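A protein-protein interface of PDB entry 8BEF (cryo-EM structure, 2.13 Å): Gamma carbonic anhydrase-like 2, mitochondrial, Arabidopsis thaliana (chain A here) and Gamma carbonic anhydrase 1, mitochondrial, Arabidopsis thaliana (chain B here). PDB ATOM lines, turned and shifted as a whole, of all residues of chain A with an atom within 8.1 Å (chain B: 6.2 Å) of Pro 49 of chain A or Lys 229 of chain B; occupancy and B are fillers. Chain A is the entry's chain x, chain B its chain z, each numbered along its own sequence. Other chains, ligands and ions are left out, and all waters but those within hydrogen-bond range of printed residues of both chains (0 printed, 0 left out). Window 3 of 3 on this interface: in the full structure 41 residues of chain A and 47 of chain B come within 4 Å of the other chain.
The side-chain hydroxyl (OG) of Ser 48 of chain A lies within hydrogen-bond range of the side-chain carboxylate (OD1) of Asp 50 of chain A, at 3.1 Å. The side-chain hydroxyl (OG) of Ser 48 of chain A lies close to the backbone NH (N) of Arg 51 of chain A (3.4 Å). NZ of Lys 229 of chain B is in salt-bridge range of OE2 of Glu 226 of chain B (3.3 Å).
Of chain B, only Lys 229 (3.9 Å) comes within 4 Å of Pro 49 of chain A. Of the printed residues of chain A, Lys 229 of chain B touches Pro 49 (3.9 Å), Asp 50 (3.7 Å) and Arg 51 (3.6 Å). Of the printed residues of chain A, Phe 227 of chain B touches Trp 54 (3.8 Å) and Tyr 56 (3.4 Å). Printed residues of chain B within 4 Å of Trp 54 of chain A: Glu 226 (3.2 Å) and Phe 227 (3.8 Å). Of the printed residues of chain B, Tyr 56 of chain A touches Phe 227 (3.4 Å), Val 230 (3.5 Å) and Leu 231 (3.5 Å). Of the printed residues of chain B, Arg 51 of chain A touches Lys 229. Of the printed residues of chain A, Val 230 of chain B touches Val 52 (3.9 Å) and Tyr 56 (3.5 Å). Ile 225 of chain B touches none of the printed residues of chain A. The nearest residue of chain B that does not touch Pro 49 of chain A is Glu 226 of chain B (6.0 Å). The nearest residue of chain A that does not touch Lys 229 of chain B is Val 52 of chain A (4.8 Å). The nearest printed residue of chain B that does not touch Val 52 of chain A is Lys 233 of chain B (4.6 Å).
NZ of Lys 229 of chain B touches O of Pro 49 of chain A, at 3.9 Å. Asp 50 of chain A touches Lys 229 of chain B. Lys 229 of chain B touches Arg 51 of chain A (NZ to O, 3.6 Å). Glu 226 of chain B touches Val 52 of chain A (OE1 to C, 3.5 Å). Val 52 of chain A touches Val 230 of chain B. Trp 54 of chain A touches Phe 227 of chain B (CZ3 to CB, 3.8 Å). CE1 of Phe 227 of chain B touches CG of Tyr 56 of chain A (3.4 Å). Tyr 56 of chain A touches Val 230 of chain B. Tyr 56 of chain A touches Leu 231 of chain B.
Of the 10 printed residues of chain A, 7 touch a printed residue of chain B. Hydrophobic or aromatic side chains of chain A that line the printed part of chain B: Val 52, Trp 54 and Tyr 56. Hydrophobic or aromatic side chains of chain B within 4 Å of the printed part of chain A: Phe 227, Val 230 and Leu 231. Among the printed residues, no Asp or Glu carboxylate lies within 4 Å of a Lys or Arg side-chain nitrogen of the other chain.
The backbone NH (N) of Lys 53 of chain A sits at hydrogen-bond distance from the side-chain carboxylate (OE1) of Glu 226 of chain B, 2.5 Å away. N of Trp 54 of chain A is in hydrogen-bond range of OE1 of Glu 226 of chain B (3.2 Å).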
ATOM      1  N   THR A  46       6.250  -9.396 -17.519  1.00  0.00           N
ATOM      2  CA  THR A  46       6.659 -10.679 -18.067  1.00  0.00           C
ATOM      3  C   THR A  46       5.583 -11.718 -17.794  1.00  0.00           C
ATOM      4  O   THR A  46       5.412 -12.136 -16.639  1.00  0.00           O
ATOM      5  CB  THR A  46       8.002 -11.118 -17.480  1.00  0.00           C
ATOM      6  OG1 THR A  46       8.484 -12.271 -18.183  1.00  0.00           O
ATOM      7  CG2 THR A  46       7.892 -11.412 -15.984  1.00  0.00           C
ATOM      8  N   PRO A  47       4.837 -12.153 -18.802  1.00  0.00           N
ATOM      9  CA  PRO A  47       3.743 -13.100 -18.573  1.00  0.00           C
ATOM     10  C   PRO A  47       4.250 -14.522 -18.378  1.00  0.00           C
ATOM     11  O   PRO A  47       5.422 -14.836 -18.579  1.00  0.00           O
ATOM     12  CB  PRO A  47       2.909 -12.987 -19.853  1.00  0.00           C
ATOM     13  CG  PRO A  47       3.876 -12.559 -20.884  1.00  0.00           C
ATOM     14  CD  PRO A  47       4.888 -11.691 -20.198  1.00  0.00           C
ATOM     15  N   SER A  48       3.322 -15.387 -17.974  1.00  0.00           N
ATOM     16  CA  SER A  48       3.560 -16.812 -17.842  1.00  0.00           C
ATOM     17  C   SER A  48       2.829 -17.567 -18.938  1.00  0.00           C
ATOM     18  O   SER A  48       1.627 -17.343 -19.139  1.00  0.00           O
ATOM     19  CB  SER A  48       3.098 -17.319 -16.474  1.00  0.00           C
ATOM     20  OG  SER A  48       1.687 -17.367 -16.392  1.00  0.00           O
ATOM     21  N   PRO A  49       3.507 -18.461 -19.661  1.00  0.00           N
ATOM     22  CA  PRO A  49       2.811 -19.249 -20.691  1.00  0.00           C
ATOM     23  C   PRO A  49       1.766 -20.195 -20.131  1.00  0.00           C
ATOM     24  O   PRO A  49       0.848 -20.577 -20.865  1.00  0.00           O
ATOM     25  CB  PRO A  49       3.949 -20.023 -21.378  1.00  0.00           C
ATOM     26  CG  PRO A  49       5.231 -19.400 -20.878  1.00  0.00           C
ATOM     27  CD  PRO A  49       4.915 -18.858 -19.523  1.00  0.00           C
ATOM     28  N   ASP A  50       1.865 -20.579 -18.861  1.00  0.00           N
ATOM     29  CA  ASP A  50       0.996 -21.601 -18.296  1.00  0.00           C
ATOM     30  C   ASP A  50      -0.237 -21.045 -17.592  1.00  0.00           C
ATOM     31  O   ASP A  50      -1.001 -21.830 -17.022  1.00  0.00           O
ATOM     32  CB  ASP A  50       1.784 -22.477 -17.317  1.00  0.00           C
ATOM     33  CG  ASP A  50       2.357 -21.692 -16.153  1.00  0.00           C
ATOM     34  OD1 ASP A  50       2.267 -20.446 -16.162  1.00  0.00           O
ATOM     35  OD2 ASP A  50       2.900 -22.324 -15.223  1.00  0.00           O
ATOM     36  N   ARG A  51      -0.459 -19.733 -17.602  1.00  0.00           N
ATOM     37  CA  ARG A  51      -1.624 -19.194 -16.909  1.00  0.00           C
ATOM     38  C   ARG A  51      -2.904 -19.609 -17.628  1.00  0.00           C
ATOM     39  O   ARG A  51      -2.987 -19.571 -18.858  1.00  0.00           O
ATOM     40  CB  ARG A  51      -1.544 -17.669 -16.796  1.00  0.00           C
ATOM     41  CG  ARG A  51      -2.908 -16.972 -16.734  1.00  0.00           C
ATOM     42  CD  ARG A  51      -2.811 -15.454 -16.794  1.00  0.00           C
ATOM     43  NE  ARG A  51      -1.830 -14.899 -15.868  1.00  0.00           N
ATOM     44  CZ  ARG A  51      -2.026 -14.745 -14.565  1.00  0.00           C
ATOM     45  NH1 ARG A  51      -3.160 -15.102 -13.987  1.00  0.00           N
ATOM     46  NH2 ARG A  51      -1.061 -14.209 -13.822  1.00  0.00           N
ATOM     47  N   VAL A  52      -3.905 -20.006 -16.847  1.00  0.00           N
ATOM     48  CA  VAL A  52      -5.147 -20.550 -17.389  1.00  0.00           C
ATOM     49  C   VAL A  52      -5.983 -19.415 -17.967  1.00  0.00           C
ATOM     50  O   VAL A  52      -6.357 -18.478 -17.254  1.00  0.00           O
ATOM     51  CB  VAL A  52      -5.931 -21.312 -16.310  1.00  0.00           C
ATOM     52  CG1 VAL A  52      -7.298 -21.742 -16.842  1.00  0.00           C
ATOM     53  CG2 VAL A  52      -5.132 -22.504 -15.817  1.00  0.00           C
ATOM     54  N   LYS A  53      -6.274 -19.498 -19.261  1.00  0.00           N
ATOM     55  CA  LYS A  53      -7.162 -18.549 -19.918  1.00  0.00           C
ATOM     56  C   LYS A  53      -8.623 -18.965 -19.804  1.00  0.00           C
ATOM     57  O   LYS A  53      -9.490 -18.123 -19.554  1.00  0.00           O
ATOM     58  CB  LYS A  53      -6.775 -18.405 -21.391  1.00  0.00           C
ATOM     59  CG  LYS A  53      -5.460 -17.683 -21.614  1.00  0.00           C
ATOM     60  CD  LYS A  53      -5.255 -17.364 -23.076  1.00  0.00           C
ATOM     61  CE  LYS A  53      -6.443 -16.607 -23.638  1.00  0.00           C
ATOM     62  NZ  LYS A  53      -6.167 -15.155 -23.752  1.00  0.00           N
ATOM     63  N   TRP A  54      -8.909 -20.253 -19.992  1.00  0.00           N
ATOM     64  CA  TRP A  54     -10.251 -20.801 -19.837  1.00  0.00           C
ATOM     65  C   TRP A  54     -10.189 -21.987 -18.889  1.00  0.00           C
ATOM     66  O   TRP A  54      -9.498 -22.972 -19.167  1.00  0.00           O
ATOM     67  CB  TRP A  54     -10.842 -21.224 -21.183  1.00  0.00           C
ATOM     68  CG  TRP A  54     -12.059 -22.089 -21.053  1.00  0.00           C
ATOM     69  CD1 TRP A  54     -13.278 -21.716 -20.572  1.00  0.00           C
ATOM     70  CD2 TRP A  54     -12.170 -23.475 -21.393  1.00  0.00           C
ATOM     71  NE1 TRP A  54     -14.143 -22.779 -20.599  1.00  0.00           N
ATOM     72  CE2 TRP A  54     -13.487 -23.874 -21.097  1.00  0.00           C
ATOM     73  CE3 TRP A  54     -11.285 -24.420 -21.919  1.00  0.00           C
ATOM     74  CZ2 TRP A  54     -13.939 -25.171 -21.307  1.00  0.00           C
ATOM     75  CZ3 TRP A  54     -11.736 -25.707 -22.133  1.00  0.00           C
ATOM     76  CH2 TRP A  54     -13.053 -26.071 -21.827  1.00  0.00           C
ATOM     77  N   TYR A  56     -12.300 -24.932 -17.392  1.00  0.00           N
ATOM     78  CA  TYR A  56     -13.526 -25.661 -17.701  1.00  0.00           C
ATOM     79  C   TYR A  56     -14.438 -25.806 -16.492  1.00  0.00           C
ATOM     80  O   TYR A  56     -15.643 -26.013 -16.662  1.00  0.00           O
ATOM     81  CB  TYR A  56     -13.199 -27.047 -18.272  1.00  0.00           C
ATOM     82  CG  TYR A  56     -12.676 -28.049 -17.262  1.00  0.00           C
ATOM     83  CD1 TYR A  56     -11.325 -28.122 -16.969  1.00  0.00           C
ATOM     84  CD2 TYR A  56     -13.534 -28.930 -16.608  1.00  0.00           C
ATOM     85  CE1 TYR A  56     -10.838 -29.033 -16.055  1.00  0.00           C
ATOM     86  CE2 TYR A  56     -13.053 -29.851 -15.689  1.00  0.00           C
ATOM     87  CZ  TYR A  56     -11.702 -29.894 -15.417  1.00  0.00           C
ATOM     88  OH  TYR A  56     -11.202 -30.798 -14.507  1.00  0.00           O
ATOM     89  N   VAL B 224      -8.707 -26.758 -26.501  1.00  0.00           N
ATOM     90  CA  VAL B 224      -8.403 -28.028 -25.858  1.00  0.00           C
ATOM     91  C   VAL B 224      -7.045 -28.009 -25.172  1.00  0.00           C
ATOM     92  O   VAL B 224      -6.814 -28.806 -24.254  1.00  0.00           O
ATOM     93  CB  VAL B 224      -8.478 -29.178 -26.878  1.00  0.00           C
ATOM     94  CG1 VAL B 224      -9.689 -29.007 -27.774  1.00  0.00           C
ATOM     95  CG2 VAL B 224      -7.210 -29.247 -27.704  1.00  0.00           C
ATOM     96  N   ILE B 225      -6.142 -27.117 -25.588  1.00  0.00           N
ATOM     97  CA  ILE B 225      -4.852 -26.991 -24.916  1.00  0.00           C
ATOM     98  C   ILE B 225      -5.038 -26.494 -23.489  1.00  0.00           C
ATOM     99  O   ILE B 225      -4.395 -26.991 -22.559  1.00  0.00           O
ATOM    100  CB  ILE B 225      -3.906 -26.075 -25.718  1.00  0.00           C
ATOM    101  CG1 ILE B 225      -3.669 -26.600 -27.143  1.00  0.00           C
ATOM    102  CG2 ILE B 225      -2.582 -25.913 -24.994  1.00  0.00           C
ATOM    103  CD1 ILE B 225      -3.786 -28.103 -27.313  1.00  0.00           C
ATOM    104  N   GLU B 226      -5.912 -25.504 -23.288  1.00  0.00           N
ATOM    105  CA  GLU B 226      -6.189 -25.037 -21.933  1.00  0.00           C
ATOM    106  C   GLU B 226      -6.806 -26.146 -21.089  1.00  0.00           C
ATOM    107  O   GLU B 226      -6.464 -26.304 -19.910  1.00  0.00           O
ATOM    108  CB  GLU B 226      -7.110 -23.817 -21.967  1.00  0.00           C
ATOM    109  CG  GLU B 226      -6.585 -22.645 -22.780  1.00  0.00           C
ATOM    110  CD  GLU B 226      -5.821 -21.635 -21.940  1.00  0.00           C
ATOM    111  OE1 GLU B 226      -6.107 -21.520 -20.730  1.00  0.00           O
ATOM    112  OE2 GLU B 226      -4.934 -20.953 -22.493  1.00  0.00           O
ATOM    113  N   PHE B 227      -7.715 -26.924 -21.680  1.00  0.00           N
ATOM    114  CA  PHE B 227      -8.314 -28.054 -20.976  1.00  0.00           C
ATOM    115  C   PHE B 227      -7.249 -29.055 -20.545  1.00  0.00           C
ATOM    116  O   PHE B 227      -7.244 -29.520 -19.400  1.00  0.00           O
ATOM    117  CB  PHE B 227      -9.360 -28.720 -21.872  1.00  0.00           C
ATOM    118  CG  PHE B 227     -10.213 -29.742 -21.169  1.00  0.00           C
ATOM    119  CD1 PHE B 227     -11.229 -29.348 -20.316  1.00  0.00           C
ATOM    120  CD2 PHE B 227     -10.009 -31.098 -21.380  1.00  0.00           C
ATOM    121  CE1 PHE B 227     -12.022 -30.284 -19.675  1.00  0.00           C
ATOM    122  CE2 PHE B 227     -10.794 -32.038 -20.742  1.00  0.00           C
ATOM    123  CZ  PHE B 227     -11.805 -31.629 -19.887  1.00  0.00           C
ATOM    124  N   GLU B 228      -6.324 -29.386 -21.451  1.00  0.00           N
ATOM    125  CA  GLU B 228      -5.259 -30.329 -21.117  1.00  0.00           C
ATOM    126  C   GLU B 228      -4.300 -29.761 -20.080  1.00  0.00           C
ATOM    127  O   GLU B 228      -3.784 -30.506 -19.241  1.00  0.00           O
ATOM    128  CB  GLU B 228      -4.498 -30.726 -22.381  1.00  0.00           C
ATOM    129  CG  GLU B 228      -5.291 -31.608 -23.320  1.00  0.00           C
ATOM    130  CD  GLU B 228      -4.627 -31.762 -24.675  1.00  0.00           C
ATOM    131  OE1 GLU B 228      -3.579 -31.123 -24.901  1.00  0.00           O
ATOM    132  OE2 GLU B 228      -5.155 -32.522 -25.514  1.00  0.00           O
ATOM    133  N   LYS B 229      -4.045 -28.453 -20.127  1.00  0.00           N
ATOM    134  CA  LYS B 229      -3.207 -27.817 -19.117  1.00  0.00           C
ATOM    135  C   LYS B 229      -3.851 -27.888 -17.739  1.00  0.00           C
ATOM    136  O   LYS B 229      -3.169 -28.128 -16.737  1.00  0.00           O
ATOM    137  CB  LYS B 229      -2.938 -26.363 -19.504  1.00  0.00           C
ATOM    138  CG  LYS B 229      -1.499 -26.077 -19.901  1.00  0.00           C
ATOM    139  CD  LYS B 229      -1.372 -24.723 -20.585  1.00  0.00           C
ATOM    140  CE  LYS B 229      -2.294 -23.688 -19.955  1.00  0.00           C
ATOM    141  NZ  LYS B 229      -2.484 -22.506 -20.835  1.00  0.00           N
ATOM    142  N   VAL B 230      -5.164 -27.668 -17.667  1.00  0.00           N
ATOM    143  CA  VAL B 230      -5.846 -27.751 -16.379  1.00  0.00           C
ATOM    144  C   VAL B 230      -5.889 -29.194 -15.888  1.00  0.00           C
ATOM    145  O   VAL B 230      -5.723 -29.461 -14.692  1.00  0.00           O
ATOM    146  CB  VAL B 230      -7.254 -27.136 -16.476  1.00  0.00           C
ATOM    147  CG1 VAL B 230      -7.978 -27.254 -15.148  1.00  0.00           C
ATOM    148  CG2 VAL B 230      -7.166 -25.680 -16.897  1.00  0.00           C
ATOM    149  N   LEU B 231      -6.112 -30.147 -16.797  1.00  0.00           N
ATOM    150  CA  LEU B 231      -6.167 -31.553 -16.402  1.00  0.00           C
ATOM    151  C   LEU B 231      -4.829 -32.039 -15.865  1.00  0.00           C
ATOM    152  O   LEU B 231      -4.777 -32.755 -14.860  1.00  0.00           O
ATOM    153  CB  LEU B 231      -6.596 -32.421 -17.584  1.00  0.00           C
ATOM    154  CG  LEU B 231      -8.049 -32.381 -18.050  1.00  0.00           C
ATOM    155  CD1 LEU B 231      -8.396 -33.684 -18.750  1.00  0.00           C
ATOM    156  CD2 LEU B 231      -8.991 -32.120 -16.887  1.00  0.00           C
ATOM    157  N   ARG B 232      -3.734 -31.663 -16.523  1.00  0.00           N
ATOM    158  CA  ARG B 232      -2.417 -32.211 -16.235  1.00  0.00           C
ATOM    159  C   ARG B 232      -1.624 -31.366 -15.242  1.00  0.00           C
ATOM    160  O   ARG B 232      -0.392 -31.465 -15.206  1.00  0.00           O
ATOM    161  CB  ARG B 232      -1.629 -32.377 -17.537  1.00  0.00           C
ATOM    162  CG  ARG B 232      -2.259 -33.356 -18.521  1.00  0.00           C
ATOM    163  CD  ARG B 232      -1.538 -33.344 -19.859  1.00  0.00           C
ATOM    164  NE  ARG B 232      -2.282 -34.067 -20.884  1.00  0.00           N
ATOM    165  CZ  ARG B 232      -1.967 -34.078 -22.173  1.00  0.00           C
ATOM    166  NH1 ARG B 232      -0.918 -33.415 -22.634  1.00  0.00           N
ATOM    167  NH2 ARG B 232      -2.724 -34.769 -23.020  1.00  0.00           N
ATOM    168  N   LYS B 233      -2.295 -30.539 -14.447  1.00  0.00           N
ATOM    169  CA  LYS B 233      -1.599 -29.723 -13.465  1.00  0.00           C
ATOM    170  C   LYS B 233      -1.067 -30.585 -12.324  1.00  0.00           C
ATOM    171  O   LYS B 233      -1.628 -31.631 -11.989  1.00  0.00           O
ATOM    172  CB  LYS B 233      -2.525 -28.639 -12.914  1.00  0.00           C
ATOM    173  CG  LYS B 233      -1.793 -27.525 -12.187  1.00  0.00           C
ATOM    174  CD  LYS B 233      -2.712 -26.375 -11.837  1.00  0.00           C
ATOM    175  CE  LYS B 233      -3.053 -25.551 -13.068  1.00  0.00           C
ATOM    176  NZ  LYS B 233      -1.833 -25.143 -13.818  1.00  0.00           N
